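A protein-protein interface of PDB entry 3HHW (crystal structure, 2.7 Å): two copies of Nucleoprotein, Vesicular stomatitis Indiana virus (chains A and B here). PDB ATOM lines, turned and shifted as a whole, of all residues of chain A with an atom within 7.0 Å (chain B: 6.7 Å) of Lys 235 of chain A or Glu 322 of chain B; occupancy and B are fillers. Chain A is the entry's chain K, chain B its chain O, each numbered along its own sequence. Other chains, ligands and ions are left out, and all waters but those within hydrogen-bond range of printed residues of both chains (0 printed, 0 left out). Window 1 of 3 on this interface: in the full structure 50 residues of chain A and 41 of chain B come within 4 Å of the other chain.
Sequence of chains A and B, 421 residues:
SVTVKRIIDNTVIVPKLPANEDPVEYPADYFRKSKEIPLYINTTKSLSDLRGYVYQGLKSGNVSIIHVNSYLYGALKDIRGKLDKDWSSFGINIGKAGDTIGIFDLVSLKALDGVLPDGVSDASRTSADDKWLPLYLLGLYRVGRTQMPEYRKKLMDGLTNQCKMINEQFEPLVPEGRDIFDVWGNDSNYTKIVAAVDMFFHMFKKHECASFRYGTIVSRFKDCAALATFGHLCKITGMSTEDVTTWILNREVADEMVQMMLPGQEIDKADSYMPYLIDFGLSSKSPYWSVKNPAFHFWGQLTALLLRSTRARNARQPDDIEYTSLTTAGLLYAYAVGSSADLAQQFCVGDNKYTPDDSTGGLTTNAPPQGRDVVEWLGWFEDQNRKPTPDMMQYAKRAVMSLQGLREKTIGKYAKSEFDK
Of the 15 printed residues of chain B, 6 touch a printed residue of chain A.
Hydrophobic or aromatic side chains of chain B that line the printed part of chain A: Tyr 323.
Along chain A the printed residues that touch a printed residue of chain B span positions 232 to 372.
Among the printed residues, 14 pairs touch across the chains.
Among the printed residues, no Asp or Glu carboxylate lies within 4 Å of a Lys or Arg side-chain nitrogen of the other chain.
A ring nitrogen (ND1) of His 232 of chain A lies within hydrogen-bond range of the side-chain carboxylate (OD1) of Asp 320 of chain B (2.6 Å).
The side-chain carboxylate (OD1) of Asp 342 of chain A is in hydrogen-bond range of the side-chain hydroxyl (OG) of Ser 325 of chain B (3.3 Å).
The side-chain carboxylate (OE2) of Glu 322 of chain B lies close to the side-chain carboxylate (OD1) of Asp 342 of chain A.
Of chain B, only Asp 320, Ile 321 and Glu 322 come within 4 Å of Lys 235 of chain A.
Glu 322 of chain B touches four residues of chain A.
Of the printed residues of chain B, Leu 307 of chain A touches Tyr 323 and Thr 324.
Printed residues of chain B within 4 Å of His 232 of chain A: Asp 320.
Printed residues of chain B within 4 Å of Ala 341 of chain A: Ser 325 (3.4 Å).
Arg 251 of chain B touches none of the printed residues of chain A.
The nearest residue of chain B that does not touch Lys 235 of chain A is Asn 20 of chain B (4.5 Å).
The nearest residue of chain A that does not touch Glu 322 of chain B is Thr 237 of chain A (4.2 Å).
The nearest printed residue of chain B that does not touch His 232 of chain A is Asp 319 of chain B (5.8 Å).
The guanidinium group (NH1) of Arg 372 of chain A sits at hydrogen-bond distance from the backbone carbonyl oxygen (O) of Thr 237 of chain A (3.2 Å).
The backbone carbonyl oxygen of Val 337 of chain A sits at hydrogen-bond distance from the guanidinium group of Arg 372 of chain A (3.1 Å).
The side-chain amide oxygen of Asn 250 of chain B lies close to the backbone carbonyl oxygen of Ser 325 of chain B.
The backbone carbonyl oxygen (O) of Tyr 323 of chain B lies within hydrogen-bond range of the side-chain hydroxyl (OG1) of Thr 327 of chain B, at 2.6 Å.
No position is printed for both chains.
Among the printed residues, pairs that only touch across the chains: Lys 235 of chain A with Asp 320 of chain B (3.5 Å), Lys 235 of chain A with Ile 321 of chain B (3.6 Å), Lys 235 of chain A with Glu 322 of chain B (3.5 Å), Ile 236 of chain A with Ile 321 of chain B (3.9 Å), Ile 236 of chain A with Glu 322 of chain B (3.5 Å), Ile 236 of chain A with Tyr 323 of chain B (3.8 Å), Gly 238 of chain A with Glu 322 of chain B (3.4 Å), Leu 307 of chain A with Tyr 323 of chain B (3.8 Å), Leu 307 of chain A with Thr 324 of chain B (3.8 Å), Ala 341 of chain A with Ser 325 of chain B (3.4 Å) and Arg 372 of chain A with Ser 325 of chain B (3.5 Å).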
ATOM      1  N   PHE A 230      18.110  13.812  18.491  1.00  0.00           N
ATOM      2  CA  PHE A 230      18.363  13.804  19.928  1.00  0.00           C
ATOM      3  C   PHE A 230      17.201  13.150  20.682  1.00  0.00           C
ATOM      4  O   PHE A 230      17.410  12.253  21.500  1.00  0.00           O
ATOM      5  CB  PHE A 230      18.606  15.248  20.403  1.00  0.00           C
ATOM      6  CG  PHE A 230      19.222  15.366  21.779  1.00  0.00           C
ATOM      7  CD1 PHE A 230      19.824  14.288  22.402  1.00  0.00           C
ATOM      8  CD2 PHE A 230      19.233  16.603  22.432  1.00  0.00           C
ATOM      9  CE1 PHE A 230      20.397  14.426  23.668  1.00  0.00           C
ATOM     10  CE2 PHE A 230      19.808  16.749  23.698  1.00  0.00           C
ATOM     11  CZ  PHE A 230      20.390  15.659  24.313  1.00  0.00           C
ATOM     12  N   GLY A 231      15.980  13.593  20.390  1.00  0.00           N
ATOM     13  CA  GLY A 231      14.784  13.033  21.017  1.00  0.00           C
ATOM     14  C   GLY A 231      14.666  11.540  20.788  1.00  0.00           C
ATOM     15  O   GLY A 231      14.366  10.781  21.707  1.00  0.00           O
ATOM     16  N   HIS A 232      14.925  11.130  19.550  1.00  0.00           N
ATOM     17  CA  HIS A 232      14.862   9.732  19.149  1.00  0.00           C
ATOM     18  C   HIS A 232      15.889   8.898  19.910  1.00  0.00           C
ATOM     19  O   HIS A 232      15.584   7.796  20.371  1.00  0.00           O
ATOM     20  CB  HIS A 232      15.072   9.616  17.637  1.00  0.00           C
ATOM     21  CG  HIS A 232      14.905   8.229  17.100  1.00  0.00           C
ATOM     22  ND1 HIS A 232      13.752   7.495  17.272  1.00  0.00           N
ATOM     23  CD2 HIS A 232      15.740   7.452  16.368  1.00  0.00           C
ATOM     24  CE1 HIS A 232      13.887   6.321  16.682  1.00  0.00           C
ATOM     25  NE2 HIS A 232      15.083   6.270  16.124  1.00  0.00           N
ATOM     26  N   LEU A 233      17.098   9.438  20.047  1.00  0.00           N
ATOM     27  CA  LEU A 233      18.171   8.769  20.766  1.00  0.00           C
ATOM     28  C   LEU A 233      17.821   8.540  22.238  1.00  0.00           C
ATOM     29  O   LEU A 233      18.197   7.523  22.813  1.00  0.00           O
ATOM     30  CB  LEU A 233      19.483   9.547  20.628  1.00  0.00           C
ATOM     31  CG  LEU A 233      20.782   8.834  21.036  1.00  0.00           C
ATOM     32  CD1 LEU A 233      20.949   7.490  20.323  1.00  0.00           C
ATOM     33  CD2 LEU A 233      21.979   9.727  20.774  1.00  0.00           C
ATOM     34  N   CYS A 234      17.089   9.480  22.833  1.00  0.00           N
ATOM     35  CA  CYS A 234      16.626   9.346  24.210  1.00  0.00           C
ATOM     36  C   CYS A 234      15.587   8.233  24.371  1.00  0.00           C
ATOM     37  O   CYS A 234      15.731   7.375  25.249  1.00  0.00           O
ATOM     38  CB  CYS A 234      16.078  10.677  24.727  1.00  0.00           C
ATOM     39  SG  CYS A 234      17.333  11.972  24.886  1.00  0.00           S
ATOM     40  N   LYS A 235      14.558   8.245  23.519  1.00  0.00           N
ATOM     41  CA  LYS A 235      13.502   7.230  23.540  1.00  0.00           C
ATOM     42  C   LYS A 235      14.054   5.821  23.329  1.00  0.00           C
ATOM     43  O   LYS A 235      13.605   4.867  23.970  1.00  0.00           O
ATOM     44  CB  LYS A 235      12.455   7.499  22.456  1.00  0.00           C
ATOM     45  CG  LYS A 235      11.785   8.869  22.489  1.00  0.00           C
ATOM     46  CD  LYS A 235      10.548   8.911  23.377  1.00  0.00           C
ATOM     47  CE  LYS A 235       9.793  10.218  23.138  1.00  0.00           C
ATOM     48  NZ  LYS A 235       8.810  10.536  24.216  1.00  0.00           N
ATOM     49  N   ILE A 236      15.029   5.695  22.432  1.00  0.00           N
ATOM     50  CA  ILE A 236      15.524   4.382  22.018  1.00  0.00           C
ATOM     51  C   ILE A 236      16.482   3.749  23.031  1.00  0.00           C
ATOM     52  O   ILE A 236      16.569   2.526  23.119  1.00  0.00           O
ATOM     53  CB  ILE A 236      16.137   4.422  20.587  1.00  0.00           C
ATOM     54  CG1 ILE A 236      16.105   3.037  19.948  1.00  0.00           C
ATOM     55  CG2 ILE A 236      17.551   5.005  20.591  1.00  0.00           C
ATOM     56  CD1 ILE A 236      15.875   3.065  18.454  1.00  0.00           C
ATOM     57  N   THR A 237      17.186   4.581  23.795  1.00  0.00           N
ATOM     58  CA  THR A 237      18.113   4.096  24.816  1.00  0.00           C
ATOM     59  C   THR A 237      17.426   3.989  26.173  1.00  0.00           C
ATOM     60  O   THR A 237      17.894   3.268  27.053  1.00  0.00           O
ATOM     61  CB  THR A 237      19.359   5.003  24.956  1.00  0.00           C
ATOM     62  OG1 THR A 237      18.956   6.330  25.306  1.00  0.00           O
ATOM     63  CG2 THR A 237      20.160   5.042  23.667  1.00  0.00           C
ATOM     64  N   GLY A 238      16.318   4.714  26.330  1.00  0.00           N
ATOM     65  CA  GLY A 238      15.591   4.784  27.604  1.00  0.00           C
ATOM     66  C   GLY A 238      16.227   5.742  28.598  1.00  0.00           C
ATOM     67  O   GLY A 238      15.805   5.828  29.754  1.00  0.00           O
ATOM     68  N   MET A 239      17.232   6.479  28.131  1.00  0.00           N
ATOM     69  CA  MET A 239      18.047   7.341  28.975  1.00  0.00           C
ATOM     70  C   MET A 239      17.614   8.802  28.892  1.00  0.00           C
ATOM     71  O   MET A 239      17.094   9.255  27.865  1.00  0.00           O
ATOM     72  CB  MET A 239      19.520   7.199  28.586  1.00  0.00           C
ATOM     73  CG  MET A 239      20.068   5.787  28.784  1.00  0.00           C
ATOM     74  SD  MET A 239      21.619   5.452  27.923  1.00  0.00           S
ATOM     75  CE  MET A 239      22.799   6.313  28.958  1.00  0.00           C
ATOM     76  N   VAL A 244      22.423  10.846  28.119  1.00  0.00           N
ATOM     77  CA  VAL A 244      22.828  10.705  26.722  1.00  0.00           C
ATOM     78  C   VAL A 244      23.997  11.645  26.438  1.00  0.00           C
ATOM     79  O   VAL A 244      24.997  11.248  25.843  1.00  0.00           O
ATOM     80  CB  VAL A 244      21.646  10.986  25.758  1.00  0.00           C
ATOM     81  CG1 VAL A 244      22.128  11.248  24.331  1.00  0.00           C
ATOM     82  CG2 VAL A 244      20.649   9.844  25.792  1.00  0.00           C
ATOM     83  N   LEU A 307      20.774   0.002  17.623  1.00  0.00           N
ATOM     84  CA  LEU A 307      19.793  -0.342  18.651  1.00  0.00           C
ATOM     85  C   LEU A 307      18.395  -0.605  18.080  1.00  0.00           C
ATOM     86  O   LEU A 307      17.395  -0.449  18.779  1.00  0.00           O
ATOM     87  CB  LEU A 307      19.743   0.734  19.735  1.00  0.00           C
ATOM     88  CG  LEU A 307      20.952   0.792  20.672  1.00  0.00           C
ATOM     89  CD1 LEU A 307      20.936   2.087  21.478  1.00  0.00           C
ATOM     90  CD2 LEU A 307      21.021  -0.434  21.586  1.00  0.00           C
ATOM     91  N   VAL A 337      24.321  -0.135  25.887  1.00  0.00           N
ATOM     92  CA  VAL A 337      22.861  -0.154  26.012  1.00  0.00           C
ATOM     93  C   VAL A 337      22.289  -1.568  25.813  1.00  0.00           C
ATOM     94  O   VAL A 337      21.470  -2.031  26.613  1.00  0.00           O
ATOM     95  CB  VAL A 337      22.199   0.827  25.007  1.00  0.00           C
ATOM     96  CG1 VAL A 337      20.690   0.834  25.165  1.00  0.00           C
ATOM     97  CG2 VAL A 337      22.751   2.229  25.183  1.00  0.00           C
ATOM     98  N   ALA A 341      20.152  -4.406  29.829  1.00  0.00           N
ATOM     99  CA  ALA A 341      18.708  -4.240  29.898  1.00  0.00           C
ATOM    100  C   ALA A 341      18.339  -3.772  31.297  1.00  0.00           C
ATOM    101  O   ALA A 341      19.061  -4.067  32.251  1.00  0.00           O
ATOM    102  CB  ALA A 341      18.019  -5.549  29.571  1.00  0.00           C
ATOM    103  N   ASP A 342      17.238  -3.027  31.425  1.00  0.00           N
ATOM    104  CA  ASP A 342      16.787  -2.563  32.747  1.00  0.00           C
ATOM    105  C   ASP A 342      16.620  -3.779  33.650  1.00  0.00           C
ATOM    106  O   ASP A 342      17.454  -4.049  34.514  1.00  0.00           O
ATOM    107  CB  ASP A 342      15.456  -1.805  32.664  1.00  0.00           C
ATOM    108  CG  ASP A 342      15.466  -0.703  31.625  1.00  0.00           C
ATOM    109  OD1 ASP A 342      14.889  -0.923  30.534  1.00  0.00           O
ATOM    110  OD2 ASP A 342      16.044   0.376  31.899  1.00  0.00           O
ATOM    111  N   ARG A 372      25.215   1.298  32.796  1.00  0.00           N
ATOM    112  CA  ARG A 372      25.430   2.136  31.613  1.00  0.00           C
ATOM    113  C   ARG A 372      26.269   3.385  31.909  1.00  0.00           C
ATOM    114  O   ARG A 372      26.236   4.360  31.157  1.00  0.00           O
ATOM    115  CB  ARG A 372      24.091   2.525  30.982  1.00  0.00           C
ATOM    116  CG  ARG A 372      23.402   1.398  30.250  1.00  0.00           C
ATOM    117  CD  ARG A 372      21.938   1.716  30.047  1.00  0.00           C
ATOM    118  NE  ARG A 372      21.274   0.717  29.215  1.00  0.00           N
ATOM    119  CZ  ARG A 372      19.972   0.706  28.949  1.00  0.00           C
ATOM    120  NH1 ARG A 372      19.175   1.636  29.456  1.00  0.00           N
ATOM    121  NH2 ARG A 372      19.462  -0.245  28.182  1.00  0.00           N
ATOM    122  N   ASN B  20       6.545  17.821  25.018  1.00  0.00           N
ATOM    123  CA  ASN B  20       5.535  16.910  24.491  1.00  0.00           C
ATOM    124  C   ASN B  20       4.494  16.551  25.557  1.00  0.00           C
ATOM    125  O   ASN B  20       4.615  15.528  26.250  1.00  0.00           O
ATOM    126  CB  ASN B  20       6.183  15.650  23.904  1.00  0.00           C
ATOM    127  CG  ASN B  20       5.177  14.741  23.210  1.00  0.00           C
ATOM    128  OD1 ASN B  20       4.122  15.191  22.750  1.00  0.00           O
ATOM    129  ND2 ASN B  20       5.505  13.452  23.128  1.00  0.00           N
ATOM    130  N   ASN B 250      10.044  -3.805  32.914  1.00  0.00           N
ATOM    131  CA  ASN B 250      10.484  -2.518  32.391  1.00  0.00           C
ATOM    132  C   ASN B 250       9.668  -1.378  32.978  1.00  0.00           C
ATOM    133  O   ASN B 250       8.448  -1.487  33.148  1.00  0.00           O
ATOM    134  CB  ASN B 250      10.386  -2.478  30.868  1.00  0.00           C
ATOM    135  CG  ASN B 250      10.817  -3.774  30.221  1.00  0.00           C
ATOM    136  OD1 ASN B 250      11.906  -3.859  29.651  1.00  0.00           O
ATOM    137  ND2 ASN B 250       9.961  -4.796  30.302  1.00  0.00           N
ATOM    138  N   ARG B 251      10.360  -0.280  33.269  1.00  0.00           N
ATOM    139  CA  ARG B 251       9.775   0.893  33.901  1.00  0.00           C
ATOM    140  C   ARG B 251       8.691   1.547  33.037  1.00  0.00           C
ATOM    141  O   ARG B 251       7.632   1.909  33.554  1.00  0.00           O
ATOM    142  CB  ARG B 251      10.880   1.893  34.246  1.00  0.00           C
ATOM    143  CG  ARG B 251      10.457   3.050  35.123  1.00  0.00           C
ATOM    144  CD  ARG B 251      11.522   4.144  35.098  1.00  0.00           C
ATOM    145  NE  ARG B 251      11.661   4.743  33.767  1.00  0.00           N
ATOM    146  CZ  ARG B 251      11.275   5.977  33.443  1.00  0.00           C
ATOM    147  NH1 ARG B 251      10.728   6.779  34.353  1.00  0.00           N
ATOM    148  NH2 ARG B 251      11.447   6.417  32.199  1.00  0.00           N
ATOM    149  N   GLU B 252       8.949   1.695  31.736  1.00  0.00           N
ATOM    150  CA  GLU B 252       7.972   2.321  30.837  1.00  0.00           C
ATOM    151  C   GLU B 252       6.667   1.541  30.746  1.00  0.00           C
ATOM    152  O   GLU B 252       5.589   2.141  30.676  1.00  0.00           O
ATOM    153  CB  GLU B 252       8.555   2.563  29.443  1.00  0.00           C
ATOM    154  CG  GLU B 252       9.137   3.960  29.249  1.00  0.00           C
ATOM    155  CD  GLU B 252       8.073   5.054  29.189  1.00  0.00           C
ATOM    156  OE1 GLU B 252       6.959   4.795  28.680  1.00  0.00           O
ATOM    157  OE2 GLU B 252       8.356   6.182  29.647  1.00  0.00           O
ATOM    158  N   ALA B 295       5.191   0.722  24.655  1.00  0.00           N
ATOM    159  CA  ALA B 295       6.069  -0.246  25.314  1.00  0.00           C
ATOM    160  C   ALA B 295       5.309  -1.510  25.713  1.00  0.00           C
ATOM    161  O   ALA B 295       5.746  -2.625  25.401  1.00  0.00           O
ATOM    162  CB  ALA B 295       6.745   0.374  26.512  1.00  0.00           C
ATOM    163  N   PHE B 298       4.371  -3.387  22.589  1.00  0.00           N
ATOM    164  CA  PHE B 298       5.490  -4.126  22.031  1.00  0.00           C
ATOM    165  C   PHE B 298       5.809  -5.342  22.897  1.00  0.00           C
ATOM    166  O   PHE B 298       5.772  -6.476  22.414  1.00  0.00           O
ATOM    167  CB  PHE B 298       6.703  -3.212  21.886  1.00  0.00           C
ATOM    168  CG  PHE B 298       7.913  -3.887  21.306  1.00  0.00           C
ATOM    169  CD1 PHE B 298       8.028  -4.080  19.935  1.00  0.00           C
ATOM    170  CD2 PHE B 298       8.946  -4.316  22.133  1.00  0.00           C
ATOM    171  CE1 PHE B 298       9.154  -4.700  19.397  1.00  0.00           C
ATOM    172  CE2 PHE B 298      10.065  -4.929  21.605  1.00  0.00           C
ATOM    173  CZ  PHE B 298      10.170  -5.123  20.236  1.00  0.00           C
ATOM    174  N   ASP B 319       7.096   3.055  17.223  1.00  0.00           N
ATOM    175  CA  ASP B 319       8.335   3.826  17.171  1.00  0.00           C
ATOM    176  C   ASP B 319       8.729   4.324  18.568  1.00  0.00           C
ATOM    177  O   ASP B 319       7.938   4.242  19.515  1.00  0.00           O
ATOM    178  CB  ASP B 319       8.192   5.016  16.214  1.00  0.00           C
ATOM    179  CG  ASP B 319       7.833   4.593  14.798  1.00  0.00           C
ATOM    180  OD1 ASP B 319       8.357   3.561  14.323  1.00  0.00           O
ATOM    181  OD2 ASP B 319       7.025   5.299  14.156  1.00  0.00           O
ATOM    182  N   ASP B 320       9.962   4.817  18.684  1.00  0.00           N
ATOM    183  CA  ASP B 320      10.429   5.544  19.868  1.00  0.00           C
ATOM    184  C   ASP B 320      10.209   4.819  21.201  1.00  0.00           C
ATOM    185  O   ASP B 320       9.644   5.372  22.144  1.00  0.00           O
ATOM    186  CB  ASP B 320       9.813   6.947  19.899  1.00  0.00           C
ATOM    187  CG  ASP B 320      10.142   7.751  18.660  1.00  0.00           C
ATOM    188  OD1 ASP B 320      11.273   7.615  18.148  1.00  0.00           O
ATOM    189  OD2 ASP B 320       9.271   8.517  18.196  1.00  0.00           O
ATOM    190  N   ILE B 321      10.657   3.569  21.252  1.00  0.00           N
ATOM    191  CA  ILE B 321      10.642   2.763  22.469  1.00  0.00           C
ATOM    192  C   ILE B 321      11.968   2.016  22.573  1.00  0.00           C
ATOM    193  O   ILE B 321      12.655   1.818  21.571  1.00  0.00           O
ATOM    194  CB  ILE B 321       9.467   1.751  22.489  1.00  0.00           C
ATOM    195  CG1 ILE B 321       9.429   0.937  21.189  1.00  0.00           C
ATOM    196  CG2 ILE B 321       8.140   2.470  22.726  1.00  0.00           C
ATOM    197  CD1 ILE B 321       8.670  -0.351  21.288  1.00  0.00           C
ATOM    198  N   GLU B 322      12.325   1.601  23.779  1.00  0.00           N
ATOM    199  CA  GLU B 322      13.590   0.916  23.990  1.00  0.00           C
ATOM    200  C   GLU B 322      13.490  -0.573  23.638  1.00  0.00           C
ATOM    201  O   GLU B 322      13.273  -1.429  24.509  1.00  0.00           O
ATOM    202  CB  GLU B 322      14.091   1.142  25.418  1.00  0.00           C
ATOM    203  CG  GLU B 322      12.988   1.315  26.454  1.00  0.00           C
ATOM    204  CD  GLU B 322      13.521   1.764  27.796  1.00  0.00           C
ATOM    205  OE1 GLU B 322      12.972   2.739  28.356  1.00  0.00           O
ATOM    206  OE2 GLU B 322      14.493   1.151  28.290  1.00  0.00           O
ATOM    207  N   TYR B 323      13.666  -0.865  22.348  1.00  0.00           N
ATOM    208  CA  TYR B 323      13.496  -2.213  21.805  1.00  0.00           C
ATOM    209  C   TYR B 323      14.344  -3.281  22.489  1.00  0.00           C
ATOM    210  O   TYR B 323      13.842  -4.369  22.778  1.00  0.00           O
ATOM    211  CB  TYR B 323      13.793  -2.243  20.302  1.00  0.00           C
ATOM    212  CG  TYR B 323      12.987  -1.286  19.466  1.00  0.00           C
ATOM    213  CD1 TYR B 323      11.658  -1.552  19.152  1.00  0.00           C
ATOM    214  CD2 TYR B 323      13.565  -0.120  18.967  1.00  0.00           C
ATOM    215  CE1 TYR B 323      10.918  -0.671  18.369  1.00  0.00           C
ATOM    216  CE2 TYR B 323      12.837   0.766  18.188  1.00  0.00           C
ATOM    217  CZ  TYR B 323      11.516   0.485  17.894  1.00  0.00           C
ATOM    218  OH  TYR B 323      10.797   1.364  17.122  1.00  0.00           O
ATOM    219  N   THR B 324      15.620  -2.984  22.733  1.00  0.00           N
ATOM    220  CA  THR B 324      16.540  -4.015  23.233  1.00  0.00           C
ATOM    221  C   THR B 324      16.177  -4.529  24.631  1.00  0.00           C
ATOM    222  O   THR B 324      16.259  -5.728  24.881  1.00  0.00           O
ATOM    223  CB  THR B 324      18.034  -3.597  23.173  1.00  0.00           C
ATOM    224  OG1 THR B 324      18.268  -2.485  24.041  1.00  0.00           O
ATOM    225  CG2 THR B 324      18.449  -3.245  21.755  1.00  0.00           C
ATOM    226  N   SER B 325      15.762  -3.627  25.520  1.00  0.00           N
ATOM    227  CA  SER B 325      15.360  -3.997  26.881  1.00  0.00           C
ATOM    228  C   SER B 325      14.025  -4.740  26.941  1.00  0.00           C
ATOM    229  O   SER B 325      13.864  -5.678  27.733  1.00  0.00           O
ATOM    230  CB  SER B 325      15.289  -2.764  27.774  1.00  0.00           C
ATOM    231  OG  SER B 325      16.586  -2.304  28.088  1.00  0.00           O
ATOM    232  N   LEU B 326      13.072  -4.316  26.113  1.00  0.00           N
ATOM    233  CA  LEU B 326      11.752  -4.929  26.096  1.00  0.00           C
ATOM    234  C   LEU B 326      11.838  -6.329  25.493  1.00  0.00           C
ATOM    235  O   LEU B 326      11.063  -7.216  25.851  1.00  0.00           O
ATOM    236  CB  LEU B 326      10.749  -4.057  25.329  1.00  0.00           C
ATOM    237  CG  LEU B 326      10.555  -2.598  25.788  1.00  0.00           C
ATOM    238  CD1 LEU B 326       9.914  -1.737  24.709  1.00  0.00           C
ATOM    239  CD2 LEU B 326       9.754  -2.509  27.081  1.00  0.00           C
ATOM    240  N   THR B 327      12.794  -6.518  24.590  1.00  0.00           N
ATOM    241  CA  THR B 327      13.032  -7.817  23.984  1.00  0.00           C
ATOM    242  C   THR B 327      13.555  -8.821  25.019  1.00  0.00           C
ATOM    243  O   THR B 327      13.019  -9.926  25.125  1.00  0.00           O
ATOM    244  CB  THR B 327      13.979  -7.706  22.761  1.00  0.00           C
ATOM    245  OG1 THR B 327      13.441  -6.757  21.830  1.00  0.00           O
ATOM    246  CG2 THR B 327      14.135  -9.044  22.060  1.00  0.00           C
